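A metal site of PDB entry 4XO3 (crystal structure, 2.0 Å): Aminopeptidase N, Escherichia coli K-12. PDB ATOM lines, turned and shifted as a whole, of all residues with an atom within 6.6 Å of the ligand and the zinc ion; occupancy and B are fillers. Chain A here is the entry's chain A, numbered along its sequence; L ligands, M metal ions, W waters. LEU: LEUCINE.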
ATOM      1  N   GLN A 115      -1.465 -19.487  11.383  1.00  0.00           N
ATOM      2  CA  GLN A 115      -2.423 -19.987  12.407  1.00  0.00           C
ATOM      3  C   GLN A 115      -1.600 -20.912  13.283  1.00  0.00           C
ATOM      4  O   GLN A 115      -1.101 -21.962  12.819  1.00  0.00           O
ATOM      5  CB  GLN A 115      -3.664 -20.690  11.811  1.00  0.00           C
ATOM      6  CG  GLN A 115      -4.516 -21.358  12.881  1.00  0.00           C
ATOM      7  CD  GLN A 115      -4.987 -20.350  13.942  1.00  0.00           C
ATOM      8  OE1 GLN A 115      -5.245 -19.194  13.651  1.00  0.00           O
ATOM      9  NE2 GLN A 115      -5.136 -20.813  15.173  1.00  0.00           N
ATOM     10  N   GLU A 117      -2.523 -21.672  16.855  1.00  0.00           N
ATOM     11  CA  GLU A 117      -3.276 -22.464  17.849  1.00  0.00           C
ATOM     12  C   GLU A 117      -3.840 -23.732  17.165  1.00  0.00           C
ATOM     13  O   GLU A 117      -4.417 -23.604  16.082  1.00  0.00           O
ATOM     14  CB  GLU A 117      -4.411 -21.646  18.487  1.00  0.00           C
ATOM     15  CG  GLU A 117      -4.980 -22.346  19.711  1.00  0.00           C
ATOM     16  CD  GLU A 117      -6.129 -21.652  20.408  1.00  0.00           C
ATOM     17  OE1 GLU A 117      -6.454 -20.522  20.012  1.00  0.00           O
ATOM     18  OE2 GLU A 117      -6.620 -22.250  21.397  1.00  0.00           O
ATOM     19  N   ALA A 118      -3.710 -24.925  17.766  1.00  0.00           N
ATOM     20  CA  ALA A 118      -3.059 -25.173  19.071  1.00  0.00           C
ATOM     21  C   ALA A 118      -1.555 -25.372  18.974  1.00  0.00           C
ATOM     22  O   ALA A 118      -0.816 -24.844  19.851  1.00  0.00           O
ATOM     23  CB  ALA A 118      -3.647 -26.454  19.683  1.00  0.00           C
ATOM     24  N   TYR A 181       1.379 -20.122  20.777  1.00  0.00           N
ATOM     25  CA  TYR A 181       0.118 -20.224  20.007  1.00  0.00           C
ATOM     26  C   TYR A 181      -0.468 -18.852  19.697  1.00  0.00           C
ATOM     27  O   TYR A 181      -1.311 -18.757  18.802  1.00  0.00           O
ATOM     28  CB  TYR A 181      -0.952 -21.137  20.601  1.00  0.00           C
ATOM     29  CG  TYR A 181      -1.761 -20.544  21.775  1.00  0.00           C
ATOM     30  CD1 TYR A 181      -2.942 -19.824  21.546  1.00  0.00           C
ATOM     31  CD2 TYR A 181      -1.347 -20.724  23.143  1.00  0.00           C
ATOM     32  CE1 TYR A 181      -3.675 -19.298  22.599  1.00  0.00           C
ATOM     33  CE2 TYR A 181      -2.084 -20.172  24.171  1.00  0.00           C
ATOM     34  CZ  TYR A 181      -3.241 -19.439  23.898  1.00  0.00           C
ATOM     35  OH  TYR A 181      -3.963 -18.896  24.910  1.00  0.00           O
ATOM     36  N   PHE A 254      -9.140 -19.990   5.969  1.00  0.00           N
ATOM     37  CA  PHE A 254      -9.001 -20.111   7.418  1.00  0.00           C
ATOM     38  C   PHE A 254      -9.847 -21.304   7.832  1.00  0.00           C
ATOM     39  O   PHE A 254     -11.022 -21.384   7.490  1.00  0.00           O
ATOM     40  CB  PHE A 254      -9.483 -18.825   8.098  1.00  0.00           C
ATOM     41  CG  PHE A 254      -9.004 -18.651   9.496  1.00  0.00           C
ATOM     42  CD1 PHE A 254      -7.633 -18.335   9.750  1.00  0.00           C
ATOM     43  CD2 PHE A 254      -9.864 -18.865  10.585  1.00  0.00           C
ATOM     44  CE1 PHE A 254      -7.194 -18.187  11.026  1.00  0.00           C
ATOM     45  CE2 PHE A 254      -9.381 -18.757  11.875  1.00  0.00           C
ATOM     46  CZ  PHE A 254      -8.036 -18.424  12.096  1.00  0.00           C
ATOM     47  N   MET A 256     -10.931 -22.168  10.886  1.00  0.00           N
ATOM     48  CA  MET A 256     -11.896 -21.957  11.990  1.00  0.00           C
ATOM     49  C   MET A 256     -12.601 -20.611  11.799  1.00  0.00           C
ATOM     50  O   MET A 256     -12.880 -20.181  10.668  1.00  0.00           O
ATOM     51  CB  MET A 256     -11.092 -22.068  13.306  1.00  0.00           C
ATOM     52  CG  MET A 256     -10.405 -23.425  13.504  1.00  0.00           C
ATOM     53  SD  MET A 256     -11.729 -24.485  14.098  1.00  0.00           S
ATOM     54  CE  MET A 256     -12.127 -23.878  15.804  1.00  0.00           C
ATOM     55  N   GLY A 257     -12.943 -19.945  12.884  1.00  0.00           N
ATOM     56  CA  GLY A 257     -13.680 -18.707  12.842  1.00  0.00           C
ATOM     57  C   GLY A 257     -12.736 -17.513  12.905  1.00  0.00           C
ATOM     58  O   GLY A 257     -12.741 -16.652  12.050  1.00  0.00           O
ATOM     59  N   ALA A 258     -12.043 -17.394  14.001  1.00  0.00           N
ATOM     60  CA  ALA A 258     -11.094 -16.300  14.165  1.00  0.00           C
ATOM     61  C   ALA A 258     -10.141 -16.600  15.301  1.00  0.00           C
ATOM     62  O   ALA A 258     -10.360 -17.527  16.098  1.00  0.00           O
ATOM     63  CB  ALA A 258     -11.808 -14.983  14.406  1.00  0.00           C
ATOM     64  N   MET A 259      -9.097 -15.778  15.436  1.00  0.00           N
ATOM     65  CA  MET A 259      -7.990 -16.090  16.344  1.00  0.00           C
ATOM     66  C   MET A 259      -7.450 -14.869  17.061  1.00  0.00           C
ATOM     67  O   MET A 259      -7.168 -13.819  16.428  1.00  0.00           O
ATOM     68  CB  MET A 259      -6.904 -16.778  15.602  1.00  0.00           C
ATOM     69  CG  MET A 259      -5.652 -17.071  16.413  1.00  0.00           C
ATOM     70  SD  MET A 259      -6.094 -18.390  17.622  1.00  0.00           S
ATOM     71  CE  MET A 259      -4.942 -17.957  18.922  1.00  0.00           C
ATOM     72  N   GLU A 260      -7.339 -15.021  18.355  1.00  0.00           N
ATOM     73  CA  GLU A 260      -7.033 -13.900  19.327  1.00  0.00           C
ATOM     74  C   GLU A 260      -5.541 -13.518  19.450  1.00  0.00           C
ATOM     75  O   GLU A 260      -5.091 -13.052  20.527  1.00  0.00           O
ATOM     76  CB  GLU A 260      -7.610 -14.184  20.689  1.00  0.00           C
ATOM     77  CG  GLU A 260      -6.921 -15.327  21.501  1.00  0.00           C
ATOM     78  CD  GLU A 260      -7.553 -16.710  21.233  1.00  0.00           C
ATOM     79  OE1 GLU A 260      -8.228 -16.960  20.183  1.00  0.00           O
ATOM     80  OE2 GLU A 260      -7.303 -17.610  22.100  1.00  0.00           O
ATOM     81  N   HIS A 293     -15.753 -11.885  20.847  1.00  0.00           N
ATOM     82  CA  HIS A 293     -15.096 -13.085  21.375  1.00  0.00           C
ATOM     83  C   HIS A 293     -13.592 -12.936  21.355  1.00  0.00           C
ATOM     84  O   HIS A 293     -12.943 -13.109  22.393  1.00  0.00           O
ATOM     85  CB  HIS A 293     -15.562 -14.335  20.562  1.00  0.00           C
ATOM     86  CG  HIS A 293     -15.011 -15.633  21.022  1.00  0.00           C
ATOM     87  ND1 HIS A 293     -15.691 -16.479  21.868  1.00  0.00           N
ATOM     88  CD2 HIS A 293     -13.819 -16.230  20.781  1.00  0.00           C
ATOM     89  CE1 HIS A 293     -14.906 -17.479  22.215  1.00  0.00           C
ATOM     90  NE2 HIS A 293     -13.791 -17.379  21.529  1.00  0.00           N
ATOM     91  N   GLU A 294     -13.017 -12.682  20.185  1.00  0.00           N
ATOM     92  CA  GLU A 294     -11.554 -12.566  20.084  1.00  0.00           C
ATOM     93  C   GLU A 294     -11.004 -11.427  20.928  1.00  0.00           C
ATOM     94  O   GLU A 294      -9.979 -11.557  21.555  1.00  0.00           O
ATOM     95  CB  GLU A 294     -11.104 -12.521  18.657  1.00  0.00           C
ATOM     96  CG  GLU A 294     -11.708 -13.622  17.759  1.00  0.00           C
ATOM     97  CD  GLU A 294     -11.556 -15.038  18.217  1.00  0.00           C
ATOM     98  OE1 GLU A 294     -10.667 -15.306  18.995  1.00  0.00           O
ATOM     99  OE2 GLU A 294     -12.373 -15.876  17.779  1.00  0.00           O
ATOM    100  N   HIS A 297     -10.825 -12.444  24.577  1.00  0.00           N
ATOM    101  CA  HIS A 297      -9.742 -13.296  24.880  1.00  0.00           C
ATOM    102  C   HIS A 297      -8.496 -12.486  25.343  1.00  0.00           C
ATOM    103  O   HIS A 297      -7.539 -13.025  25.920  1.00  0.00           O
ATOM    104  CB  HIS A 297      -9.332 -14.076  23.650  1.00  0.00           C
ATOM    105  CG  HIS A 297      -9.969 -15.423  23.490  1.00  0.00           C
ATOM    106  ND1 HIS A 297      -9.955 -16.375  24.483  1.00  0.00           N
ATOM    107  CD2 HIS A 297     -10.606 -15.985  22.427  1.00  0.00           C
ATOM    108  CE1 HIS A 297     -10.590 -17.464  24.051  1.00  0.00           C
ATOM    109  NE2 HIS A 297     -10.960 -17.252  22.811  1.00  0.00           N
ATOM    110  N   LEU A 312      -8.202 -26.019  27.917  1.00  0.00           N
ATOM    111  CA  LEU A 312      -8.705 -25.158  26.872  1.00  0.00           C
ATOM    112  C   LEU A 312      -9.996 -24.421  27.282  1.00  0.00           C
ATOM    113  O   LEU A 312     -10.153 -23.221  26.991  1.00  0.00           O
ATOM    114  CB  LEU A 312      -8.971 -25.936  25.594  1.00  0.00           C
ATOM    115  CG  LEU A 312      -9.498 -25.178  24.387  1.00  0.00           C
ATOM    116  CD1 LEU A 312      -8.555 -24.023  23.984  1.00  0.00           C
ATOM    117  CD2 LEU A 312      -9.690 -26.106  23.188  1.00  0.00           C
ATOM    118  N   LYS A 315     -10.145 -20.798  28.890  1.00  0.00           N
ATOM    119  CA  LYS A 315     -10.279 -19.626  28.059  1.00  0.00           C
ATOM    120  C   LYS A 315     -11.516 -19.744  27.163  1.00  0.00           C
ATOM    121  O   LYS A 315     -12.197 -18.717  26.944  1.00  0.00           O
ATOM    122  CB  LYS A 315      -9.011 -19.307  27.267  1.00  0.00           C
ATOM    123  CG  LYS A 315      -8.590 -20.261  26.148  1.00  0.00           C
ATOM    124  CD  LYS A 315      -7.281 -19.761  25.504  1.00  0.00           C
ATOM    125  CE  LYS A 315      -6.845 -20.558  24.307  1.00  0.00           C
ATOM    126  NZ  LYS A 315      -7.550 -20.354  23.035  1.00  0.00           N
ATOM    127  N   GLU A 316     -11.832 -20.946  26.632  1.00  0.00           N
ATOM    128  CA  GLU A 316     -12.928 -20.975  25.617  1.00  0.00           C
ATOM    129  C   GLU A 316     -14.309 -20.879  26.251  1.00  0.00           C
ATOM    130  O   GLU A 316     -15.147 -20.147  25.743  1.00  0.00           O
ATOM    131  CB  GLU A 316     -12.838 -22.089  24.576  1.00  0.00           C
ATOM    132  CG  GLU A 316     -11.561 -22.036  23.773  1.00  0.00           C
ATOM    133  CD  GLU A 316     -11.400 -20.751  23.000  1.00  0.00           C
ATOM    134  OE1 GLU A 316     -12.448 -20.071  22.745  1.00  0.00           O
ATOM    135  OE2 GLU A 316     -10.263 -20.543  22.519  1.00  0.00           O
ATOM    136  N   THR A 319     -14.643 -17.307  27.570  1.00  0.00           N
ATOM    137  CA  THR A 319     -14.755 -16.318  26.537  1.00  0.00           C
ATOM    138  C   THR A 319     -16.085 -16.437  25.766  1.00  0.00           C
ATOM    139  O   THR A 319     -16.648 -15.420  25.355  1.00  0.00           O
ATOM    140  CB  THR A 319     -13.547 -16.344  25.639  1.00  0.00           C
ATOM    141  OG1 THR A 319     -12.399 -16.101  26.460  1.00  0.00           O
ATOM    142  CG2 THR A 319     -13.602 -15.271  24.561  1.00  0.00           C
ATOM    143  N   VAL A 320     -16.583 -17.654  25.572  1.00  0.00           N
ATOM    144  CA  VAL A 320     -17.930 -17.829  25.027  1.00  0.00           C
ATOM    145  C   VAL A 320     -18.962 -17.205  25.946  1.00  0.00           C
ATOM    146  O   VAL A 320     -19.860 -16.508  25.497  1.00  0.00           O
ATOM    147  CB  VAL A 320     -18.262 -19.315  24.774  1.00  0.00           C
ATOM    148  CG1 VAL A 320     -19.758 -19.454  24.412  1.00  0.00           C
ATOM    149  CG2 VAL A 320     -17.402 -19.833  23.662  1.00  0.00           C
ATOM    150  N   ASN A 369      -6.379 -30.533  18.009  1.00  0.00           N
ATOM    151  CA  ASN A 369      -7.278 -29.747  17.183  1.00  0.00           C
ATOM    152  C   ASN A 369      -8.644 -30.401  17.091  1.00  0.00           C
ATOM    153  O   ASN A 369      -9.605 -29.713  16.678  1.00  0.00           O
ATOM    154  CB  ASN A 369      -6.730 -29.374  15.794  1.00  0.00           C
ATOM    155  CG  ASN A 369      -5.503 -28.420  15.880  1.00  0.00           C
ATOM    156  OD1 ASN A 369      -4.417 -28.718  15.376  1.00  0.00           O
ATOM    157  ND2 ASN A 369      -5.649 -27.405  16.569  1.00  0.00           N
ATOM    158  N   TYR A 372     -11.616 -28.645  19.874  1.00  0.00           N
ATOM    159  CA  TYR A 372     -12.200 -27.308  19.743  1.00  0.00           C
ATOM    160  C   TYR A 372     -13.689 -27.526  19.492  1.00  0.00           C
ATOM    161  O   TYR A 372     -14.188 -27.316  18.384  1.00  0.00           O
ATOM    162  CB  TYR A 372     -11.453 -26.504  18.644  1.00  0.00           C
ATOM    163  CG  TYR A 372     -10.131 -26.045  19.206  1.00  0.00           C
ATOM    164  CD1 TYR A 372      -9.043 -26.895  19.282  1.00  0.00           C
ATOM    165  CD2 TYR A 372      -9.973 -24.767  19.679  1.00  0.00           C
ATOM    166  CE1 TYR A 372      -7.890 -26.535  19.961  1.00  0.00           C
ATOM    167  CE2 TYR A 372      -8.801 -24.355  20.292  1.00  0.00           C
ATOM    168  CZ  TYR A 372      -7.717 -25.235  20.369  1.00  0.00           C
ATOM    169  OH  TYR A 372      -6.576 -24.872  21.021  1.00  0.00           O
ATOM    170  N   TYR A 377     -16.496 -25.406  24.194  1.00  0.00           N
ATOM    171  CA  TYR A 377     -16.942 -24.041  23.993  1.00  0.00           C
ATOM    172  C   TYR A 377     -18.329 -23.792  24.660  1.00  0.00           C
ATOM    173  O   TYR A 377     -18.443 -23.008  25.619  1.00  0.00           O
ATOM    174  CB  TYR A 377     -17.024 -23.735  22.535  1.00  0.00           C
ATOM    175  CG  TYR A 377     -15.739 -23.359  21.910  1.00  0.00           C
ATOM    176  CD1 TYR A 377     -14.709 -24.264  21.779  1.00  0.00           C
ATOM    177  CD2 TYR A 377     -15.561 -22.066  21.403  1.00  0.00           C
ATOM    178  CE1 TYR A 377     -13.494 -23.924  21.173  1.00  0.00           C
ATOM    179  CE2 TYR A 377     -14.381 -21.732  20.762  1.00  0.00           C
ATOM    180  CZ  TYR A 377     -13.331 -22.637  20.650  1.00  0.00           C
ATOM    181  OH  TYR A 377     -12.155 -22.284  20.055  1.00  0.00           O
ATOM    182  N   ARG A 821     -13.582 -32.177  11.024  1.00  0.00           N
ATOM    183  CA  ARG A 821     -14.900 -31.564  11.233  1.00  0.00           C
ATOM    184  C   ARG A 821     -15.996 -32.225  10.390  1.00  0.00           C
ATOM    185  O   ARG A 821     -17.088 -32.496  10.894  1.00  0.00           O
ATOM    186  CB  ARG A 821     -14.864 -30.036  10.870  1.00  0.00           C
ATOM    187  CG  ARG A 821     -13.986 -29.199  11.761  1.00  0.00           C
ATOM    188  CD  ARG A 821     -14.682 -28.879  13.070  1.00  0.00           C
ATOM    189  NE  ARG A 821     -13.879 -27.936  13.850  1.00  0.00           N
ATOM    190  CZ  ARG A 821     -13.965 -27.727  15.190  1.00  0.00           C
ATOM    191  NH1 ARG A 821     -13.165 -26.870  15.777  1.00  0.00           N
ATOM    192  NH2 ARG A 821     -14.859 -28.311  15.912  1.00  0.00           N
HETATM  193  N   LEU L   1      -8.798 -19.564  19.798  1.00  0.00           N
HETATM  194  CA  LEU L   1      -9.728 -19.669  18.630  1.00  0.00           C
HETATM  195  C   LEU L   1     -11.120 -19.348  19.113  1.00  0.00           C
HETATM  196  O   LEU L   1     -11.266 -18.416  19.889  1.00  0.00           O
HETATM  197  CB  LEU L   1      -9.684 -21.066  18.027  1.00  0.00           C
HETATM  198  CG  LEU L   1      -8.455 -21.339  17.106  1.00  0.00           C
HETATM  199  CD1 LEU L   1      -8.186 -22.845  16.966  1.00  0.00           C
HETATM  200  CD2 LEU L   1      -8.748 -20.684  15.748  1.00  0.00           C
HETATM  201  OXT LEU L   1     -12.133 -19.991  18.723  1.00  0.00           O
HETATM  202 ZN    ZN M   1     -12.145 -18.463  21.702  1.00  0.00          ZN
HETATM  203  O   HOH W   1     -12.665 -19.889  15.784  1.00  0.00           O
HETATM  204  O   HOH W   2      -7.894 -25.844  16.402  1.00  0.00           O
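The side-chain carboxylate of Glu 260 is in salt-bridge range of a nitrogen (N) of the ligand (2.7 Å).
N of the ligand is in salt-bridge range of OE1 of Glu 117 (2.5 Å).
OH of Tyr 377 lies within hydrogen-bond range of OXT of the ligand (2.7 Å).
SD of Met 259 is in hydrogen-bond range of N of the ligand (3.7 Å).
The side-chain amide nitrogen (NE2) of Gln 115 sits at hydrogen-bond distance from the side-chain sulfur (SD) of Met 259 (3.6 Å).
SD of Met 256 lies close to NH1 of Arg 821.
The side-chain carboxylate of Glu 294 sits at hydrogen-bond distance from the backbone NH of Glu 260 (3.4 Å).
The backbone carbonyl oxygen (O) of Tyr 372 lies within hydrogen-bond range of the guanidinium group (NH2) of Arg 821.
A ring nitrogen (ND1) of His 297 sits at hydrogen-bond distance from the side-chain hydroxyl of Thr 319 (3.2 Å).
NZ of Lys 315 is in salt-bridge range of OE2 of Glu 260.
The side-chain carboxylate of Glu 316 is in salt-bridge range of the side-chain amino group of Lys 315 (2.8 Å).
OH of Tyr 377 lies close to OE1 of Glu 316 (3.5 Å).
The side-chain carboxylate of Glu 294 lies close to an oxygen (O) of the ligand, at 3.3 Å.
Merely in contact with the ligand: Gln 115 (3.7 Å), Met 256 (3.7 Å), Ala 258 (3.4 Å), Lys 315 (3.6 Å) and Tyr 372 (3.7 Å).
Hydrophobic or aromatic side chains that line the ligand: Met 256, Met 259, His 293, His 297, Tyr 372 and Tyr 377.
Within 4 Å of the zinc ion: His 293, His 297 and Glu 316.
The nearest printed residue that does not touch the zinc ion is Tyr 377 (4.1 Å).
The zinc ion is bound by the side-chain carboxylate of Glu 316 (1.9 Å), a ring nitrogen (NE2) of His 293 (2.0 Å), an oxygen (O) of the ligand (2.0 Å) and a ring nitrogen (NE2) of His 297 (2.0 Å).
The zinc ion has four donor atoms within binding distance.
Water W1 lies within hydrogen-bond range of N of Gly 257, OXT of the ligand and N of Ala 258.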
